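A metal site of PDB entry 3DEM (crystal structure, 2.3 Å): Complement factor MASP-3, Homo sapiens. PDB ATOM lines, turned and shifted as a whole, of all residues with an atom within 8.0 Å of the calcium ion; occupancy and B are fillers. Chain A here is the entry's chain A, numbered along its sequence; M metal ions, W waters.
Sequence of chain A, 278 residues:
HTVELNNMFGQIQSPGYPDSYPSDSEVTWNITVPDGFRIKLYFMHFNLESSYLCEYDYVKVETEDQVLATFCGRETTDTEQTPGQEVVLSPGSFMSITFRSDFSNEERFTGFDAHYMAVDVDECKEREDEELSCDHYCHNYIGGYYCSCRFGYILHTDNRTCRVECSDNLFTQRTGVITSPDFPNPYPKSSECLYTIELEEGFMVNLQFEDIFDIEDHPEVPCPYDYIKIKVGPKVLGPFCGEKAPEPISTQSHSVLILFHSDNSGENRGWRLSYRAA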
ATOM      1  N   ASP A  35      -5.910  -8.103   2.938  1.00  0.00           N
ATOM      2  CA  ASP A  35      -5.813  -7.804   1.511  1.00  0.00           C
ATOM      3  C   ASP A  35      -7.137  -8.136   0.821  1.00  0.00           C
ATOM      4  O   ASP A  35      -7.794  -9.122   1.164  1.00  0.00           O
ATOM      5  CB  ASP A  35      -4.669  -8.578   0.871  1.00  0.00           C
ATOM      6  CG  ASP A  35      -3.308  -8.123   1.374  1.00  0.00           C
ATOM      7  OD1 ASP A  35      -3.217  -7.014   1.947  1.00  0.00           O
ATOM      8  OD2 ASP A  35      -2.321  -8.874   1.195  1.00  0.00           O
ATOM      9  N   GLY A  36      -7.508  -7.315  -0.157  1.00  0.00           N
ATOM     10  CA  GLY A  36      -8.755  -7.506  -0.875  1.00  0.00           C
ATOM     11  C   GLY A  36      -9.913  -6.739  -0.243  1.00  0.00           C
ATOM     12  O   GLY A  36     -11.044  -6.832  -0.703  1.00  0.00           O
ATOM     13  N   PHE A  37      -9.610  -5.992   0.809  1.00  0.00           N
ATOM     14  CA  PHE A  37     -10.621  -5.174   1.484  1.00  0.00           C
ATOM     15  C   PHE A  37     -10.211  -3.707   1.529  1.00  0.00           C
ATOM     16  O   PHE A  37      -9.031  -3.383   1.488  1.00  0.00           O
ATOM     17  CB  PHE A  37     -10.859  -5.670   2.908  1.00  0.00           C
ATOM     18  CG  PHE A  37     -11.441  -7.046   2.993  1.00  0.00           C
ATOM     19  CD1 PHE A  37     -12.810  -7.246   2.958  1.00  0.00           C
ATOM     20  CD2 PHE A  37     -10.618  -8.148   3.133  1.00  0.00           C
ATOM     21  CE1 PHE A  37     -13.343  -8.518   3.043  1.00  0.00           C
ATOM     22  CE2 PHE A  37     -11.146  -9.425   3.225  1.00  0.00           C
ATOM     23  CZ  PHE A  37     -12.510  -9.599   3.175  1.00  0.00           C
ATOM     24  N   VAL A 119     -14.690  -3.412   3.645  1.00  0.00           N
ATOM     25  CA  VAL A 119     -15.547  -3.531   2.478  1.00  0.00           C
ATOM     26  C   VAL A 119     -14.793  -4.292   1.401  1.00  0.00           C
ATOM     27  O   VAL A 119     -13.643  -3.968   1.097  1.00  0.00           O
ATOM     28  CB  VAL A 119     -15.944  -2.147   1.916  1.00  0.00           C
ATOM     29  CG1 VAL A 119     -16.798  -2.299   0.678  1.00  0.00           C
ATOM     30  CG2 VAL A 119     -16.689  -1.357   2.990  1.00  0.00           C
ATOM     31  N   ASP A 120     -15.417  -5.313   0.835  1.00  0.00           N
ATOM     32  CA  ASP A 120     -14.770  -6.096  -0.207  1.00  0.00           C
ATOM     33  C   ASP A 120     -14.457  -5.255  -1.432  1.00  0.00           C
ATOM     34  O   ASP A 120     -15.292  -4.486  -1.896  1.00  0.00           O
ATOM     35  CB  ASP A 120     -15.628  -7.286  -0.626  1.00  0.00           C
ATOM     36  CG  ASP A 120     -14.997  -8.079  -1.753  1.00  0.00           C
ATOM     37  OD1 ASP A 120     -13.838  -8.512  -1.578  1.00  0.00           O
ATOM     38  OD2 ASP A 120     -15.646  -8.264  -2.802  1.00  0.00           O
ATOM     39  N   VAL A 121     -13.238  -5.409  -1.948  1.00  0.00           N
ATOM     40  CA  VAL A 121     -12.860  -4.838  -3.229  1.00  0.00           C
ATOM     41  C   VAL A 121     -13.429  -5.720  -4.324  1.00  0.00           C
ATOM     42  O   VAL A 121     -13.224  -6.939  -4.311  1.00  0.00           O
ATOM     43  CB  VAL A 121     -11.320  -4.763  -3.377  1.00  0.00           C
ATOM     44  CG1 VAL A 121     -10.931  -4.365  -4.794  1.00  0.00           C
ATOM     45  CG2 VAL A 121     -10.734  -3.795  -2.358  1.00  0.00           C
ATOM     46  N   ASP A 122     -14.150  -5.130  -5.264  1.00  0.00           N
ATOM     47  CA  ASP A 122     -14.582  -5.859  -6.446  1.00  0.00           C
ATOM     48  C   ASP A 122     -13.532  -5.680  -7.546  1.00  0.00           C
ATOM     49  O   ASP A 122     -13.597  -4.746  -8.335  1.00  0.00           O
ATOM     50  CB  ASP A 122     -15.955  -5.385  -6.934  1.00  0.00           C
ATOM     51  CG  ASP A 122     -16.530  -6.262  -8.035  1.00  0.00           C
ATOM     52  OD1 ASP A 122     -15.752  -6.992  -8.697  1.00  0.00           O
ATOM     53  OD2 ASP A 122     -17.751  -6.234  -8.235  1.00  0.00           O
ATOM     54  N   GLU A 123     -12.562  -6.594  -7.583  1.00  0.00           N
ATOM     55  CA  GLU A 123     -11.441  -6.478  -8.516  1.00  0.00           C
ATOM     56  C   GLU A 123     -11.893  -6.543  -9.961  1.00  0.00           C
ATOM     57  O   GLU A 123     -11.228  -6.030 -10.854  1.00  0.00           O
ATOM     58  CB  GLU A 123     -10.386  -7.562  -8.250  1.00  0.00           C
ATOM     59  CG  GLU A 123      -9.646  -7.434  -6.926  1.00  0.00           C
ATOM     60  CD  GLU A 123     -10.309  -8.208  -5.782  1.00  0.00           C
ATOM     61  OE1 GLU A 123     -11.450  -8.661  -5.946  1.00  0.00           O
ATOM     62  OE2 GLU A 123      -9.674  -8.355  -4.717  1.00  0.00           O
ATOM     63  N   CYS A 124     -13.047  -7.180 -10.201  1.00  0.00           N
ATOM     64  CA  CYS A 124     -13.575  -7.313 -11.550  1.00  0.00           C
ATOM     65  C   CYS A 124     -14.077  -5.974 -12.096  1.00  0.00           C
ATOM     66  O   CYS A 124     -14.091  -5.764 -13.305  1.00  0.00           O
ATOM     67  CB  CYS A 124     -14.676  -8.360 -11.602  1.00  0.00           C
ATOM     68  SG  CYS A 124     -14.125  -9.989 -11.022  1.00  0.00           S
ATOM     69  N   GLU A 126     -13.083  -2.775 -10.367  1.00  0.00           N
ATOM     70  CA  GLU A 126     -12.079  -1.776 -10.034  1.00  0.00           C
ATOM     71  C   GLU A 126     -10.683  -2.180 -10.493  1.00  0.00           C
ATOM     72  O   GLU A 126     -10.509  -2.689 -11.615  1.00  0.00           O
ATOM     73  CB  GLU A 126     -12.088  -1.544  -8.514  1.00  0.00           C
ATOM     74  CG  GLU A 126     -13.491  -1.559  -7.895  1.00  0.00           C
ATOM     75  CD  GLU A 126     -13.467  -1.627  -6.379  1.00  0.00           C
ATOM     76  OE1 GLU A 126     -12.465  -1.176  -5.787  1.00  0.00           O
ATOM     77  OE2 GLU A 126     -14.452  -2.137  -5.777  1.00  0.00           O
ATOM     78  N   HIS A 139     -14.461 -13.365 -11.759  1.00  0.00           N
ATOM     79  CA  HIS A 139     -15.432 -13.688 -10.713  1.00  0.00           C
ATOM     80  C   HIS A 139     -14.979 -13.079  -9.393  1.00  0.00           C
ATOM     81  O   HIS A 139     -13.893 -13.380  -8.889  1.00  0.00           O
ATOM     82  CB  HIS A 139     -15.583 -15.209 -10.555  1.00  0.00           C
ATOM     83  CG  HIS A 139     -15.899 -15.921 -11.830  1.00  0.00           C
ATOM     84  ND1 HIS A 139     -17.181 -16.168 -12.251  1.00  0.00           N
ATOM     85  CD2 HIS A 139     -15.079 -16.448 -12.779  1.00  0.00           C
ATOM     86  CE1 HIS A 139     -17.154 -16.815 -13.403  1.00  0.00           C
ATOM     87  NE2 HIS A 139     -15.892 -16.998 -13.750  1.00  0.00           N
ATOM     88  N   ASN A 140     -15.810 -12.205  -8.838  1.00  0.00           N
ATOM     89  CA  ASN A 140     -15.497 -11.574  -7.574  1.00  0.00           C
ATOM     90  C   ASN A 140     -16.024 -12.381  -6.393  1.00  0.00           C
ATOM     91  O   ASN A 140     -17.107 -12.969  -6.478  1.00  0.00           O
ATOM     92  CB  ASN A 140     -16.090 -10.160  -7.510  1.00  0.00           C
ATOM     93  CG  ASN A 140     -15.642  -9.389  -6.282  1.00  0.00           C
ATOM     94  OD1 ASN A 140     -14.455  -9.383  -5.934  1.00  0.00           O
ATOM     95  ND2 ASN A 140     -16.573  -8.730  -5.625  1.00  0.00           N
ATOM     96  N   TYR A 141     -15.246 -12.416  -5.328  1.00  0.00           N
ATOM     97  CA  TYR A 141     -15.728 -12.929  -4.049  1.00  0.00           C
ATOM     98  C   TYR A 141     -15.178 -12.094  -2.895  1.00  0.00           C
ATOM     99  O   TYR A 141     -14.360 -11.189  -3.106  1.00  0.00           O
ATOM    100  CB  TYR A 141     -15.400 -14.422  -3.872  1.00  0.00           C
ATOM    101  CG  TYR A 141     -13.920 -14.751  -3.787  1.00  0.00           C
ATOM    102  CD1 TYR A 141     -13.237 -14.687  -2.581  1.00  0.00           C
ATOM    103  CD2 TYR A 141     -13.230 -15.158  -4.915  1.00  0.00           C
ATOM    104  CE1 TYR A 141     -11.884 -14.993  -2.503  1.00  0.00           C
ATOM    105  CE2 TYR A 141     -11.881 -15.475  -4.856  1.00  0.00           C
ATOM    106  CZ  TYR A 141     -11.219 -15.390  -3.646  1.00  0.00           C
ATOM    107  OH  TYR A 141      -9.885 -15.706  -3.589  1.00  0.00           O
ATOM    108  N   ILE A 142     -15.635 -12.383  -1.689  1.00  0.00           N
ATOM    109  CA  ILE A 142     -15.244 -11.627  -0.512  1.00  0.00           C
ATOM    110  C   ILE A 142     -13.801 -11.942  -0.139  1.00  0.00           C
ATOM    111  O   ILE A 142     -13.482 -13.060   0.289  1.00  0.00           O
ATOM    112  CB  ILE A 142     -16.205 -11.901   0.668  1.00  0.00           C
ATOM    113  CG1 ILE A 142     -17.626 -11.440   0.306  1.00  0.00           C
ATOM    114  CG2 ILE A 142     -15.731 -11.212   1.936  1.00  0.00           C
ATOM    115  CD1 ILE A 142     -18.695 -11.853   1.297  1.00  0.00           C
ATOM    116  N   GLY A 143     -12.918 -10.964  -0.324  1.00  0.00           N
ATOM    117  CA  GLY A 143     -11.519 -11.112   0.026  1.00  0.00           C
ATOM    118  C   GLY A 143     -10.596 -11.427  -1.136  1.00  0.00           C
ATOM    119  O   GLY A 143      -9.372 -11.408  -0.981  1.00  0.00           O
ATOM    120  N   GLY A 144     -11.169 -11.720  -2.302  1.00  0.00           N
ATOM    121  CA  GLY A 144     -10.362 -11.999  -3.486  1.00  0.00           C
ATOM    122  C   GLY A 144     -11.152 -12.040  -4.779  1.00  0.00           C
ATOM    123  O   GLY A 144     -12.245 -11.493  -4.868  1.00  0.00           O
ATOM    124  N   TYR A 145     -10.572 -12.682  -5.796  1.00  0.00           N
ATOM    125  CA  TYR A 145     -11.243 -12.884  -7.084  1.00  0.00           C
ATOM    126  C   TYR A 145     -10.510 -13.996  -7.830  1.00  0.00           C
ATOM    127  O   TYR A 145      -9.431 -14.414  -7.421  1.00  0.00           O
ATOM    128  CB  TYR A 145     -11.252 -11.592  -7.905  1.00  0.00           C
ATOM    129  CG  TYR A 145      -9.919 -11.273  -8.560  1.00  0.00           C
ATOM    130  CD1 TYR A 145      -9.704 -11.554  -9.903  1.00  0.00           C
ATOM    131  CD2 TYR A 145      -8.889 -10.699  -7.828  1.00  0.00           C
ATOM    132  CE1 TYR A 145      -8.488 -11.268 -10.509  1.00  0.00           C
ATOM    133  CE2 TYR A 145      -7.673 -10.406  -8.428  1.00  0.00           C
ATOM    134  CZ  TYR A 145      -7.474 -10.695  -9.762  1.00  0.00           C
ATOM    135  OH  TYR A 145      -6.270 -10.407 -10.340  1.00  0.00           O
ATOM    136  N   TYR A 146     -11.108 -14.480  -8.915  1.00  0.00           N
ATOM    137  CA  TYR A 146     -10.436 -15.428  -9.810  1.00  0.00           C
ATOM    138  C   TYR A 146     -10.966 -15.303 -11.229  1.00  0.00           C
ATOM    139  O   TYR A 146     -12.022 -14.701 -11.449  1.00  0.00           O
ATOM    140  CB  TYR A 146     -10.567 -16.865  -9.288  1.00  0.00           C
ATOM    141  CG  TYR A 146     -11.969 -17.420  -9.293  1.00  0.00           C
ATOM    142  CD1 TYR A 146     -12.481 -18.100 -10.398  1.00  0.00           C
ATOM    143  CD2 TYR A 146     -12.793 -17.263  -8.182  1.00  0.00           C
ATOM    144  CE1 TYR A 146     -13.766 -18.613 -10.400  1.00  0.00           C
ATOM    145  CE2 TYR A 146     -14.086 -17.772  -8.173  1.00  0.00           C
ATOM    146  CZ  TYR A 146     -14.569 -18.445  -9.285  1.00  0.00           C
ATOM    147  OH  TYR A 146     -15.848 -18.947  -9.268  1.00  0.00           O
HETATM  148 CA    CA M   1     -13.208  -9.205  -4.082  1.00  0.00          CA
HETATM  149  O   HOH W   1     -11.281  -8.819  -2.731  1.00  0.00           O
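The backbone NH of Asn 140 lies within hydrogen-bond range of the side-chain sulfur of Cys 124, at 3.5 Å.
The backbone NH of Val 121 lies within hydrogen-bond range of the backbone carbonyl oxygen of Gly 36 (2.9 Å).
The backbone NH of Gly 143 sits close to the side-chain carboxylate of Asp 120, 2.9 Å away.
Of the 18 residues printed, 6 come within 4 Å of the calcium ion.
The calcium ion is bound by OD1 of Asn 140 (2.2 Å), O of Val 121 (2.3 Å), water W1 (2.4 Å), O of Tyr 141 (2.5 Å), O of Gly 144 (2.6 Å), OE1 of Glu 123 (2.6 Å) and OD1 of Asp 120 (2.7 Å).
The calcium ion has seven donor atoms within binding distance.
Slightly farther from the calcium ion lies OD2 of Asp 120 (2.9 Å).
Water W1 lies within hydrogen-bond range of OE2 of Glu 123, O of Gly 36 and N of Gly 144.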
